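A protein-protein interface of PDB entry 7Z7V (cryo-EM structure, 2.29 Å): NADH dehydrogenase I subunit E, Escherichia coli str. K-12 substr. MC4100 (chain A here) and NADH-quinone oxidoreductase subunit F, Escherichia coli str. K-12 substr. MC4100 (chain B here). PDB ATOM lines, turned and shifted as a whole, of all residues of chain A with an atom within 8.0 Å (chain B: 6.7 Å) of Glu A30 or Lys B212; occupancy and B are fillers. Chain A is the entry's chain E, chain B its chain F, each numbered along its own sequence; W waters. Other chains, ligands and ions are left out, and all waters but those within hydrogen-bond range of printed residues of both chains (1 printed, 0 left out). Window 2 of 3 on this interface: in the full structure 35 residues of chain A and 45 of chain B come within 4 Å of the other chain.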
ATOM      1  N   GLU A  25     -22.080  24.752 -28.196  1.00  0.00           N
ATOM      2  CA  GLU A  25     -21.124  25.717 -27.662  1.00  0.00           C
ATOM      3  C   GLU A  25     -20.636  25.321 -26.274  1.00  0.00           C
ATOM      4  O   GLU A  25     -19.496  25.628 -25.912  1.00  0.00           O
ATOM      5  CB  GLU A  25     -21.737  27.112 -27.630  1.00  0.00           C
ATOM      6  CG  GLU A  25     -20.701  28.208 -27.533  1.00  0.00           C
ATOM      7  CD  GLU A  25     -19.994  28.468 -28.850  1.00  0.00           C
ATOM      8  OE1 GLU A  25     -20.506  28.037 -29.905  1.00  0.00           O
ATOM      9  OE2 GLU A  25     -18.921  29.106 -28.830  1.00  0.00           O
ATOM     10  N   MET A  26     -21.477  24.643 -25.491  1.00  0.00           N
ATOM     11  CA  MET A  26     -21.053  24.158 -24.183  1.00  0.00           C
ATOM     12  C   MET A  26     -19.976  23.090 -24.300  1.00  0.00           C
ATOM     13  O   MET A  26     -19.189  22.902 -23.367  1.00  0.00           O
ATOM     14  CB  MET A  26     -22.248  23.608 -23.407  1.00  0.00           C
ATOM     15  CG  MET A  26     -23.103  24.663 -22.744  1.00  0.00           C
ATOM     16  SD  MET A  26     -24.696  24.007 -22.219  1.00  0.00           S
ATOM     17  CE  MET A  26     -24.173  22.683 -21.139  1.00  0.00           C
ATOM     18  N   HIS A  27     -19.931  22.378 -25.429  1.00  0.00           N
ATOM     19  CA  HIS A  27     -18.868  21.399 -25.646  1.00  0.00           C
ATOM     20  C   HIS A  27     -17.486  22.034 -25.784  1.00  0.00           C
ATOM     21  O   HIS A  27     -16.483  21.347 -25.579  1.00  0.00           O
ATOM     22  CB  HIS A  27     -19.158  20.572 -26.897  1.00  0.00           C
ATOM     23  CG  HIS A  27     -20.257  19.573 -26.718  1.00  0.00           C
ATOM     24  ND1 HIS A  27     -21.065  19.165 -27.757  1.00  0.00           N
ATOM     25  CD2 HIS A  27     -20.687  18.908 -25.621  1.00  0.00           C
ATOM     26  CE1 HIS A  27     -21.944  18.286 -27.307  1.00  0.00           C
ATOM     27  NE2 HIS A  27     -21.736  18.113 -26.015  1.00  0.00           N
ATOM     28  N   HIS A  28     -17.407  23.321 -26.122  1.00  0.00           N
ATOM     29  CA  HIS A  28     -16.135  23.947 -26.460  1.00  0.00           C
ATOM     30  C   HIS A  28     -15.320  24.371 -25.246  1.00  0.00           C
ATOM     31  O   HIS A  28     -14.174  24.796 -25.413  1.00  0.00           O
ATOM     32  CB  HIS A  28     -16.372  25.170 -27.346  1.00  0.00           C
ATOM     33  CG  HIS A  28     -17.013  24.850 -28.659  1.00  0.00           C
ATOM     34  ND1 HIS A  28     -17.082  23.570 -29.163  1.00  0.00           N
ATOM     35  CD2 HIS A  28     -17.625  25.645 -29.568  1.00  0.00           C
ATOM     36  CE1 HIS A  28     -17.704  23.590 -30.327  1.00  0.00           C
ATOM     37  NE2 HIS A  28     -18.044  24.837 -30.596  1.00  0.00           N
ATOM     38  N   TYR A  29     -15.871  24.272 -24.041  1.00  0.00           N
ATOM     39  CA  TYR A  29     -15.212  24.779 -22.850  1.00  0.00           C
ATOM     40  C   TYR A  29     -15.263  23.737 -21.745  1.00  0.00           C
ATOM     41  O   TYR A  29     -16.032  22.775 -21.800  1.00  0.00           O
ATOM     42  CB  TYR A  29     -15.858  26.078 -22.361  1.00  0.00           C
ATOM     43  CG  TYR A  29     -16.077  27.111 -23.440  1.00  0.00           C
ATOM     44  CD1 TYR A  29     -15.066  27.988 -23.801  1.00  0.00           C
ATOM     45  CD2 TYR A  29     -17.301  27.222 -24.082  1.00  0.00           C
ATOM     46  CE1 TYR A  29     -15.263  28.936 -24.779  1.00  0.00           C
ATOM     47  CE2 TYR A  29     -17.507  28.166 -25.062  1.00  0.00           C
ATOM     48  CZ  TYR A  29     -16.483  29.021 -25.406  1.00  0.00           C
ATOM     49  OH  TYR A  29     -16.680  29.967 -26.382  1.00  0.00           O
ATOM     50  N   GLU A  30     -14.428  23.943 -20.733  1.00  0.00           N
ATOM     51  CA  GLU A  30     -14.390  23.076 -19.566  1.00  0.00           C
ATOM     52  C   GLU A  30     -15.390  23.484 -18.493  1.00  0.00           C
ATOM     53  O   GLU A  30     -15.478  22.813 -17.461  1.00  0.00           O
ATOM     54  CB  GLU A  30     -12.979  23.054 -18.980  1.00  0.00           C
ATOM     55  CG  GLU A  30     -12.498  24.394 -18.479  1.00  0.00           C
ATOM     56  CD  GLU A  30     -11.399  24.262 -17.452  1.00  0.00           C
ATOM     57  OE1 GLU A  30     -11.721  24.111 -16.257  1.00  0.00           O
ATOM     58  OE2 GLU A  30     -10.215  24.310 -17.837  1.00  0.00           O
ATOM     59  N   ASP A  31     -16.145  24.560 -18.715  1.00  0.00           N
ATOM     60  CA  ASP A  31     -17.150  25.034 -17.786  1.00  0.00           C
ATOM     61  C   ASP A  31     -18.307  25.529 -18.648  1.00  0.00           C
ATOM     62  O   ASP A  31     -18.089  26.351 -19.553  1.00  0.00           O
ATOM     63  CB  ASP A  31     -16.600  26.152 -16.895  1.00  0.00           C
ATOM     64  CG  ASP A  31     -17.442  26.401 -15.657  1.00  0.00           C
ATOM     65  OD1 ASP A  31     -18.682  26.321 -15.723  1.00  0.00           O
ATOM     66  OD2 ASP A  31     -16.848  26.686 -14.599  1.00  0.00           O
ATOM     67  N   PRO A  32     -19.532  25.040 -18.417  1.00  0.00           N
ATOM     68  CA  PRO A  32     -20.673  25.494 -19.233  1.00  0.00           C
ATOM     69  C   PRO A  32     -21.025  26.964 -19.063  1.00  0.00           C
ATOM     70  O   PRO A  32     -21.744  27.500 -19.914  1.00  0.00           O
ATOM     71  CB  PRO A  32     -21.823  24.590 -18.767  1.00  0.00           C
ATOM     72  CG  PRO A  32     -21.385  24.052 -17.454  1.00  0.00           C
ATOM     73  CD  PRO A  32     -19.903  23.931 -17.528  1.00  0.00           C
ATOM     74  N   ARG A  33     -20.555  27.625 -18.000  1.00  0.00           N
ATOM     75  CA  ARG A  33     -20.770  29.063 -17.846  1.00  0.00           C
ATOM     76  C   ARG A  33     -20.119  29.852 -18.976  1.00  0.00           C
ATOM     77  O   ARG A  33     -20.616  30.917 -19.358  1.00  0.00           O
ATOM     78  CB  ARG A  33     -20.227  29.524 -16.492  1.00  0.00           C
ATOM     79  CG  ARG A  33     -20.424  30.999 -16.184  1.00  0.00           C
ATOM     80  CD  ARG A  33     -19.535  31.447 -15.047  1.00  0.00           C
ATOM     81  NE  ARG A  33     -19.922  30.815 -13.793  1.00  0.00           N
ATOM     82  CZ  ARG A  33     -20.902  31.239 -13.011  1.00  0.00           C
ATOM     83  NH1 ARG A  33     -21.603  32.320 -13.307  1.00  0.00           N
ATOM     84  NH2 ARG A  33     -21.191  30.560 -11.907  1.00  0.00           N
ATOM     85  N   ALA A  34     -19.041  29.323 -19.553  1.00  0.00           N
ATOM     86  CA  ALA A  34     -18.318  29.989 -20.627  1.00  0.00           C
ATOM     87  C   ALA A  34     -19.112  30.091 -21.922  1.00  0.00           C
ATOM     88  O   ALA A  34     -18.685  30.810 -22.829  1.00  0.00           O
ATOM     89  CB  ALA A  34     -17.000  29.264 -20.876  1.00  0.00           C
ATOM     90  N   ILE B  84      -2.874  21.087 -18.095  1.00  0.00           N
ATOM     91  CA  ILE B  84      -3.960  21.759 -18.797  1.00  0.00           C
ATOM     92  C   ILE B  84      -3.559  23.214 -18.979  1.00  0.00           C
ATOM     93  O   ILE B  84      -3.403  23.949 -17.997  1.00  0.00           O
ATOM     94  CB  ILE B  84      -5.283  21.635 -18.026  1.00  0.00           C
ATOM     95  CG1 ILE B  84      -5.762  20.183 -18.017  1.00  0.00           C
ATOM     96  CG2 ILE B  84      -6.339  22.551 -18.616  1.00  0.00           C
ATOM     97  CD1 ILE B  84      -6.141  19.654 -19.377  1.00  0.00           C
ATOM     98  N   ARG B  85      -3.381  23.638 -20.229  1.00  0.00           N
ATOM     99  CA  ARG B  85      -2.873  24.974 -20.495  1.00  0.00           C
ATOM    100  C   ARG B  85      -3.597  25.615 -21.671  1.00  0.00           C
ATOM    101  O   ARG B  85      -4.032  24.944 -22.627  1.00  0.00           O
ATOM    102  CB  ARG B  85      -1.363  24.956 -20.743  1.00  0.00           C
ATOM    103  CG  ARG B  85      -0.541  24.991 -19.475  1.00  0.00           C
ATOM    104  CD  ARG B  85       0.847  24.428 -19.684  1.00  0.00           C
ATOM    105  NE  ARG B  85       1.414  23.919 -18.442  1.00  0.00           N
ATOM    106  CZ  ARG B  85       2.558  24.330 -17.914  1.00  0.00           C
ATOM    107  NH1 ARG B  85       3.294  25.259 -18.499  1.00  0.00           N
ATOM    108  NH2 ARG B  85       2.974  23.793 -16.772  1.00  0.00           N
ATOM    109  N   TYR B  86      -3.704  26.940 -21.590  1.00  0.00           N
ATOM    110  CA  TYR B  86      -4.488  27.707 -22.542  1.00  0.00           C
ATOM    111  C   TYR B  86      -3.656  28.809 -23.178  1.00  0.00           C
ATOM    112  O   TYR B  86      -2.898  29.512 -22.501  1.00  0.00           O
ATOM    113  CB  TYR B  86      -5.718  28.308 -21.872  1.00  0.00           C
ATOM    114  CG  TYR B  86      -6.705  27.266 -21.415  1.00  0.00           C
ATOM    115  CD1 TYR B  86      -7.516  26.612 -22.326  1.00  0.00           C
ATOM    116  CD2 TYR B  86      -6.819  26.931 -20.073  1.00  0.00           C
ATOM    117  CE1 TYR B  86      -8.415  25.660 -21.918  1.00  0.00           C
ATOM    118  CE2 TYR B  86      -7.718  25.978 -19.656  1.00  0.00           C
ATOM    119  CZ  TYR B  86      -8.511  25.345 -20.583  1.00  0.00           C
ATOM    120  OH  TYR B  86      -9.410  24.392 -20.175  1.00  0.00           O
ATOM    121  N   TYR B 126      -2.740  22.928 -24.409  1.00  0.00           N
ATOM    122  CA  TYR B 126      -3.628  21.981 -25.058  1.00  0.00           C
ATOM    123  C   TYR B 126      -4.784  22.669 -25.763  1.00  0.00           C
ATOM    124  O   TYR B 126      -5.335  22.098 -26.707  1.00  0.00           O
ATOM    125  CB  TYR B 126      -4.137  20.956 -24.042  1.00  0.00           C
ATOM    126  CG  TYR B 126      -5.534  21.196 -23.517  1.00  0.00           C
ATOM    127  CD1 TYR B 126      -5.785  22.201 -22.592  1.00  0.00           C
ATOM    128  CD2 TYR B 126      -6.593  20.394 -23.914  1.00  0.00           C
ATOM    129  CE1 TYR B 126      -7.051  22.419 -22.104  1.00  0.00           C
ATOM    130  CE2 TYR B 126      -7.866  20.604 -23.426  1.00  0.00           C
ATOM    131  CZ  TYR B 126      -8.086  21.615 -22.519  1.00  0.00           C
ATOM    132  OH  TYR B 126      -9.349  21.834 -22.026  1.00  0.00           O
ATOM    133  N   ARG B 127      -5.168  23.879 -25.349  1.00  0.00           N
ATOM    134  CA  ARG B 127      -6.268  24.531 -26.047  1.00  0.00           C
ATOM    135  C   ARG B 127      -5.930  25.974 -26.385  1.00  0.00           C
ATOM    136  O   ARG B 127      -5.166  26.637 -25.678  1.00  0.00           O
ATOM    137  CB  ARG B 127      -7.562  24.471 -25.236  1.00  0.00           C
ATOM    138  CG  ARG B 127      -8.571  23.487 -25.792  1.00  0.00           C
ATOM    139  CD  ARG B 127      -9.837  23.453 -24.962  1.00  0.00           C
ATOM    140  NE  ARG B 127     -10.687  22.328 -25.325  1.00  0.00           N
ATOM    141  CZ  ARG B 127     -11.693  21.879 -24.588  1.00  0.00           C
ATOM    142  NH1 ARG B 127     -12.011  22.443 -23.435  1.00  0.00           N
ATOM    143  NH2 ARG B 127     -12.399  20.839 -25.018  1.00  0.00           N
ATOM    144  N   TYR B 129      -7.815  29.718 -27.880  1.00  0.00           N
ATOM    145  CA  TYR B 129      -9.025  30.473 -28.169  1.00  0.00           C
ATOM    146  C   TYR B 129      -8.647  31.802 -28.796  1.00  0.00           C
ATOM    147  O   TYR B 129      -7.788  32.510 -28.271  1.00  0.00           O
ATOM    148  CB  TYR B 129      -9.849  30.721 -26.904  1.00  0.00           C
ATOM    149  CG  TYR B 129     -10.397  29.479 -26.246  1.00  0.00           C
ATOM    150  CD1 TYR B 129      -9.670  28.806 -25.277  1.00  0.00           C
ATOM    151  CD2 TYR B 129     -11.653  28.993 -26.579  1.00  0.00           C
ATOM    152  CE1 TYR B 129     -10.171  27.678 -24.667  1.00  0.00           C
ATOM    153  CE2 TYR B 129     -12.160  27.865 -25.976  1.00  0.00           C
ATOM    154  CZ  TYR B 129     -11.415  27.214 -25.019  1.00  0.00           C
ATOM    155  OH  TYR B 129     -11.919  26.090 -24.414  1.00  0.00           O
ATOM    156  N   PHE B 203      -0.451  36.471 -11.957  1.00  0.00           N
ATOM    157  CA  PHE B 203      -0.565  36.726 -13.378  1.00  0.00           C
ATOM    158  C   PHE B 203      -1.222  35.532 -14.061  1.00  0.00           C
ATOM    159  O   PHE B 203      -1.253  34.435 -13.499  1.00  0.00           O
ATOM    160  CB  PHE B 203       0.820  37.020 -13.947  1.00  0.00           C
ATOM    161  CG  PHE B 203       1.336  38.374 -13.569  1.00  0.00           C
ATOM    162  CD1 PHE B 203       1.027  39.483 -14.336  1.00  0.00           C
ATOM    163  CD2 PHE B 203       2.096  38.546 -12.427  1.00  0.00           C
ATOM    164  CE1 PHE B 203       1.488  40.734 -13.984  1.00  0.00           C
ATOM    165  CE2 PHE B 203       2.558  39.793 -12.069  1.00  0.00           C
ATOM    166  CZ  PHE B 203       2.252  40.888 -12.848  1.00  0.00           C
ATOM    167  N   PRO B 204      -1.794  35.724 -15.256  1.00  0.00           N
ATOM    168  CA  PRO B 204      -2.456  34.600 -15.941  1.00  0.00           C
ATOM    169  C   PRO B 204      -1.541  33.434 -16.265  1.00  0.00           C
ATOM    170  O   PRO B 204      -2.044  32.322 -16.464  1.00  0.00           O
ATOM    171  CB  PRO B 204      -3.000  35.244 -17.221  1.00  0.00           C
ATOM    172  CG  PRO B 204      -3.202  36.654 -16.864  1.00  0.00           C
ATOM    173  CD  PRO B 204      -2.111  37.010 -15.907  1.00  0.00           C
ATOM    174  N   ALA B 205      -0.224  33.651 -16.324  1.00  0.00           N
ATOM    175  CA  ALA B 205       0.711  32.565 -16.591  1.00  0.00           C
ATOM    176  C   ALA B 205       0.670  31.497 -15.505  1.00  0.00           C
ATOM    177  O   ALA B 205       0.884  30.317 -15.795  1.00  0.00           O
ATOM    178  CB  ALA B 205       2.128  33.118 -16.734  1.00  0.00           C
ATOM    179  N   THR B 206       0.387  31.879 -14.262  1.00  0.00           N
ATOM    180  CA  THR B 206       0.292  30.898 -13.190  1.00  0.00           C
ATOM    181  C   THR B 206      -1.141  30.424 -12.972  1.00  0.00           C
ATOM    182  O   THR B 206      -1.381  29.220 -12.837  1.00  0.00           O
ATOM    183  CB  THR B 206       0.870  31.468 -11.892  1.00  0.00           C
ATOM    184  OG1 THR B 206       0.410  32.811 -11.705  1.00  0.00           O
ATOM    185  CG2 THR B 206       2.385  31.472 -11.954  1.00  0.00           C
ATOM    186  N   SER B 207      -2.102  31.345 -12.939  1.00  0.00           N
ATOM    187  CA  SER B 207      -3.511  30.995 -12.755  1.00  0.00           C
ATOM    188  C   SER B 207      -4.354  31.970 -13.570  1.00  0.00           C
ATOM    189  O   SER B 207      -4.651  33.076 -13.113  1.00  0.00           O
ATOM    190  CB  SER B 207      -3.901  31.018 -11.282  1.00  0.00           C
ATOM    191  OG  SER B 207      -3.659  32.286 -10.709  1.00  0.00           O
ATOM    192  N   GLY B 208      -4.737  31.552 -14.771  1.00  0.00           N
ATOM    193  CA  GLY B 208      -5.506  32.396 -15.662  1.00  0.00           C
ATOM    194  C   GLY B 208      -6.893  31.868 -15.951  1.00  0.00           C
ATOM    195  O   GLY B 208      -7.782  31.952 -15.102  1.00  0.00           O
ATOM    196  N   ALA B 209      -7.086  31.327 -17.151  1.00  0.00           N
ATOM    197  CA  ALA B 209      -8.397  30.850 -17.573  1.00  0.00           C
ATOM    198  C   ALA B 209      -8.767  29.584 -16.814  1.00  0.00           C
ATOM    199  O   ALA B 209      -8.075  28.567 -16.920  1.00  0.00           O
ATOM    200  CB  ALA B 209      -8.407  30.604 -19.077  1.00  0.00           C
ATOM    201  N   TRP B 210      -9.859  29.663 -16.047  1.00  0.00           N
ATOM    202  CA  TRP B 210     -10.348  28.584 -15.184  1.00  0.00           C
ATOM    203  C   TRP B 210      -9.284  28.113 -14.198  1.00  0.00           C
ATOM    204  O   TRP B 210      -9.209  26.931 -13.864  1.00  0.00           O
ATOM    205  CB  TRP B 210     -10.885  27.408 -16.004  1.00  0.00           C
ATOM    206  CG  TRP B 210     -11.967  27.800 -16.957  1.00  0.00           C
ATOM    207  CD1 TRP B 210     -13.269  28.042 -16.656  1.00  0.00           C
ATOM    208  CD2 TRP B 210     -11.835  28.010 -18.366  1.00  0.00           C
ATOM    209  NE1 TRP B 210     -13.961  28.384 -17.788  1.00  0.00           N
ATOM    210  CE2 TRP B 210     -13.102  28.374 -18.854  1.00  0.00           C
ATOM    211  CE3 TRP B 210     -10.768  27.924 -19.264  1.00  0.00           C
ATOM    212  CZ2 TRP B 210     -13.334  28.651 -20.197  1.00  0.00           C
ATOM    213  CZ3 TRP B 210     -10.999  28.202 -20.596  1.00  0.00           C
ATOM    214  CH2 TRP B 210     -12.271  28.560 -21.051  1.00  0.00           C
ATOM    215  N   GLY B 211      -8.442  29.036 -13.735  1.00  0.00           N
ATOM    216  CA  GLY B 211      -7.384  28.725 -12.802  1.00  0.00           C
ATOM    217  C   GLY B 211      -6.157  28.084 -13.407  1.00  0.00           C
ATOM    218  O   GLY B 211      -5.164  27.900 -12.694  1.00  0.00           O
ATOM    219  N   LYS B 212      -6.184  27.741 -14.687  1.00  0.00           N
ATOM    220  CA  LYS B 212      -5.080  27.059 -15.335  1.00  0.00           C
ATOM    221  C   LYS B 212      -4.038  28.058 -15.818  1.00  0.00           C
ATOM    222  O   LYS B 212      -4.315  29.255 -15.921  1.00  0.00           O
ATOM    223  CB  LYS B 212      -5.594  26.231 -16.507  1.00  0.00           C
ATOM    224  CG  LYS B 212      -6.786  25.371 -16.173  1.00  0.00           C
ATOM    225  CD  LYS B 212      -6.440  24.337 -15.124  1.00  0.00           C
ATOM    226  CE  LYS B 212      -7.537  23.300 -15.009  1.00  0.00           C
ATOM    227  NZ  LYS B 212      -8.856  23.928 -14.718  1.00  0.00           N
ATOM    228  N   PRO B 213      -2.814  27.599 -16.073  1.00  0.00           N
ATOM    229  CA  PRO B 213      -1.839  28.451 -16.764  1.00  0.00           C
ATOM    230  C   PRO B 213      -2.340  28.883 -18.137  1.00  0.00           C
ATOM    231  O   PRO B 213      -2.778  28.067 -18.959  1.00  0.00           O
ATOM    232  CB  PRO B 213      -0.591  27.566 -16.863  1.00  0.00           C
ATOM    233  CG  PRO B 213      -0.864  26.349 -16.055  1.00  0.00           C
ATOM    234  CD  PRO B 213      -2.166  26.486 -15.363  1.00  0.00           C
ATOM    235  N   THR B 214      -2.265  30.186 -18.371  1.00  0.00           N
ATOM    236  CA  THR B 214      -2.856  30.832 -19.527  1.00  0.00           C
ATOM    237  C   THR B 214      -1.898  31.893 -20.034  1.00  0.00           C
ATOM    238  O   THR B 214      -1.280  32.607 -19.243  1.00  0.00           O
ATOM    239  CB  THR B 214      -4.204  31.469 -19.167  1.00  0.00           C
ATOM    240  OG1 THR B 214      -5.020  30.512 -18.484  1.00  0.00           O
ATOM    241  CG2 THR B 214      -4.926  31.947 -20.401  1.00  0.00           C
ATOM    242  N   CYS B 215      -1.762  31.992 -21.347  1.00  0.00           N
ATOM    243  CA  CYS B 215      -0.974  33.056 -21.947  1.00  0.00           C
ATOM    244  C   CYS B 215      -1.825  33.818 -22.945  1.00  0.00           C
ATOM    245  O   CYS B 215      -2.375  33.222 -23.872  1.00  0.00           O
ATOM    246  CB  CYS B 215       0.274  32.509 -22.631  1.00  0.00           C
ATOM    247  SG  CYS B 215       1.382  33.806 -23.166  1.00  0.00           S
HETATM  248  O   HOH W   1     -11.667  24.933 -21.984  1.00  0.00           O
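Water W1 lies within hydrogen-bond range of the side-chain hydroxyl of Tyr B129 (2.7 Å), the guanidinium group of Arg B127 (2.9 Å), the side-chain hydroxyl of Tyr B86 (2.9 Å) and the backbone NH of Glu A30 (3.2 Å).
The backbone carbonyl oxygen (O) of Arg B85 sits at hydrogen-bond distance from the backbone NH (N) of Arg B127 (3.1 Å).
OH of Tyr B86 lies within hydrogen-bond range of OH of Tyr B126, 3.2 Å away.
The backbone NH of Tyr B86 lies within hydrogen-bond range of the backbone carbonyl oxygen of Pro B213 (3.0 Å).
NZ of Lys B212 is in hydrogen-bond range of O of Trp B210 (3.1 Å).
The backbone carbonyl oxygen (O) of Lys B212 lies within hydrogen-bond range of the side-chain hydroxyl (OG1) of Thr B214 (2.9 Å).
The side-chain carboxylate (OE2) of Glu A25 sits at hydrogen-bond distance from the side-chain hydroxyl (OH) of Tyr A29 (3.4 Å).
The side-chain hydroxyl (OH) of Tyr B86 lies within hydrogen-bond range of the side-chain carboxylate (OE2) of Glu A30 (2.5 Å).
OH of Tyr B129 sits at hydrogen-bond distance from O of His A28 (2.8 Å).
The side-chain amino group (NZ) of Lys B212 is in salt-bridge range of the side-chain carboxylate (OE1) of Glu A30, 3.3 Å away.
Printed residues of chain A that touch a printed residue of chain B: His A28, Tyr A29, Glu A30, Asp A31 and Ala A34.
Hydrophobic or aromatic side chains of chain A that line the printed part of chain B: Tyr A29 and Ala A34.
Printed residues of chain B that touch a printed residue of chain A: Tyr B86, Arg B127, Tyr B129, Trp B210 and Lys B212.
Hydrophobic or aromatic side chains of chain B within 4 Å of the printed part of chain A: Tyr B86, Tyr B129 and Trp B210.
Among the printed residues, Asp or Glu carboxylates within 4 Å of a Lys or Arg side-chain nitrogen of the other chain: Glu A30 with Lys B212 (3.3 Å).
Of chain B, only Tyr B86 (2.5 Å), Arg B127 (3.9 Å), Trp B210 (3.4 Å) and Lys B212 (3.3 Å) come within 4 Å of Glu A30.
Lys B212 touches one residue of chain A.
No residue of chain A comes within 4 Å of Gly B211.
Of the printed residues of chain A, Tyr B86 touches Glu A30 (2.5 Å).
Of the printed residues of chain B, Ala A34 touches Trp B210.
Printed residues of chain B within 4 Å of Asp A31: Trp B210.
Of the printed residues of chain B, Tyr A29 touches Arg B127, Tyr B129 and Trp B210.
Printed residues of chain A within 4 Å of Trp B210: Tyr A29, Glu A30, Asp A31 and Ala A34.
The nearest residue of chain B that does not touch Glu A30 is Ile B84 (4.3 Å).
The nearest printed residue of chain A that does not touch Lys B212 is Asp A31 (8.3 Å).
The nearest printed residue of chain B that does not touch Ala A34 is Tyr B129 (7.0 Å).
Among the printed residues, merely in contact across the chains: His A28 with Arg B127, Tyr A29 with Arg B127, Tyr A29 with Tyr B129, Tyr A29 with Trp B210, Glu A30 with Arg B127, Glu A30 with Trp B210, Asp A31 with Trp B210 and Ala A34 with Trp B210.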
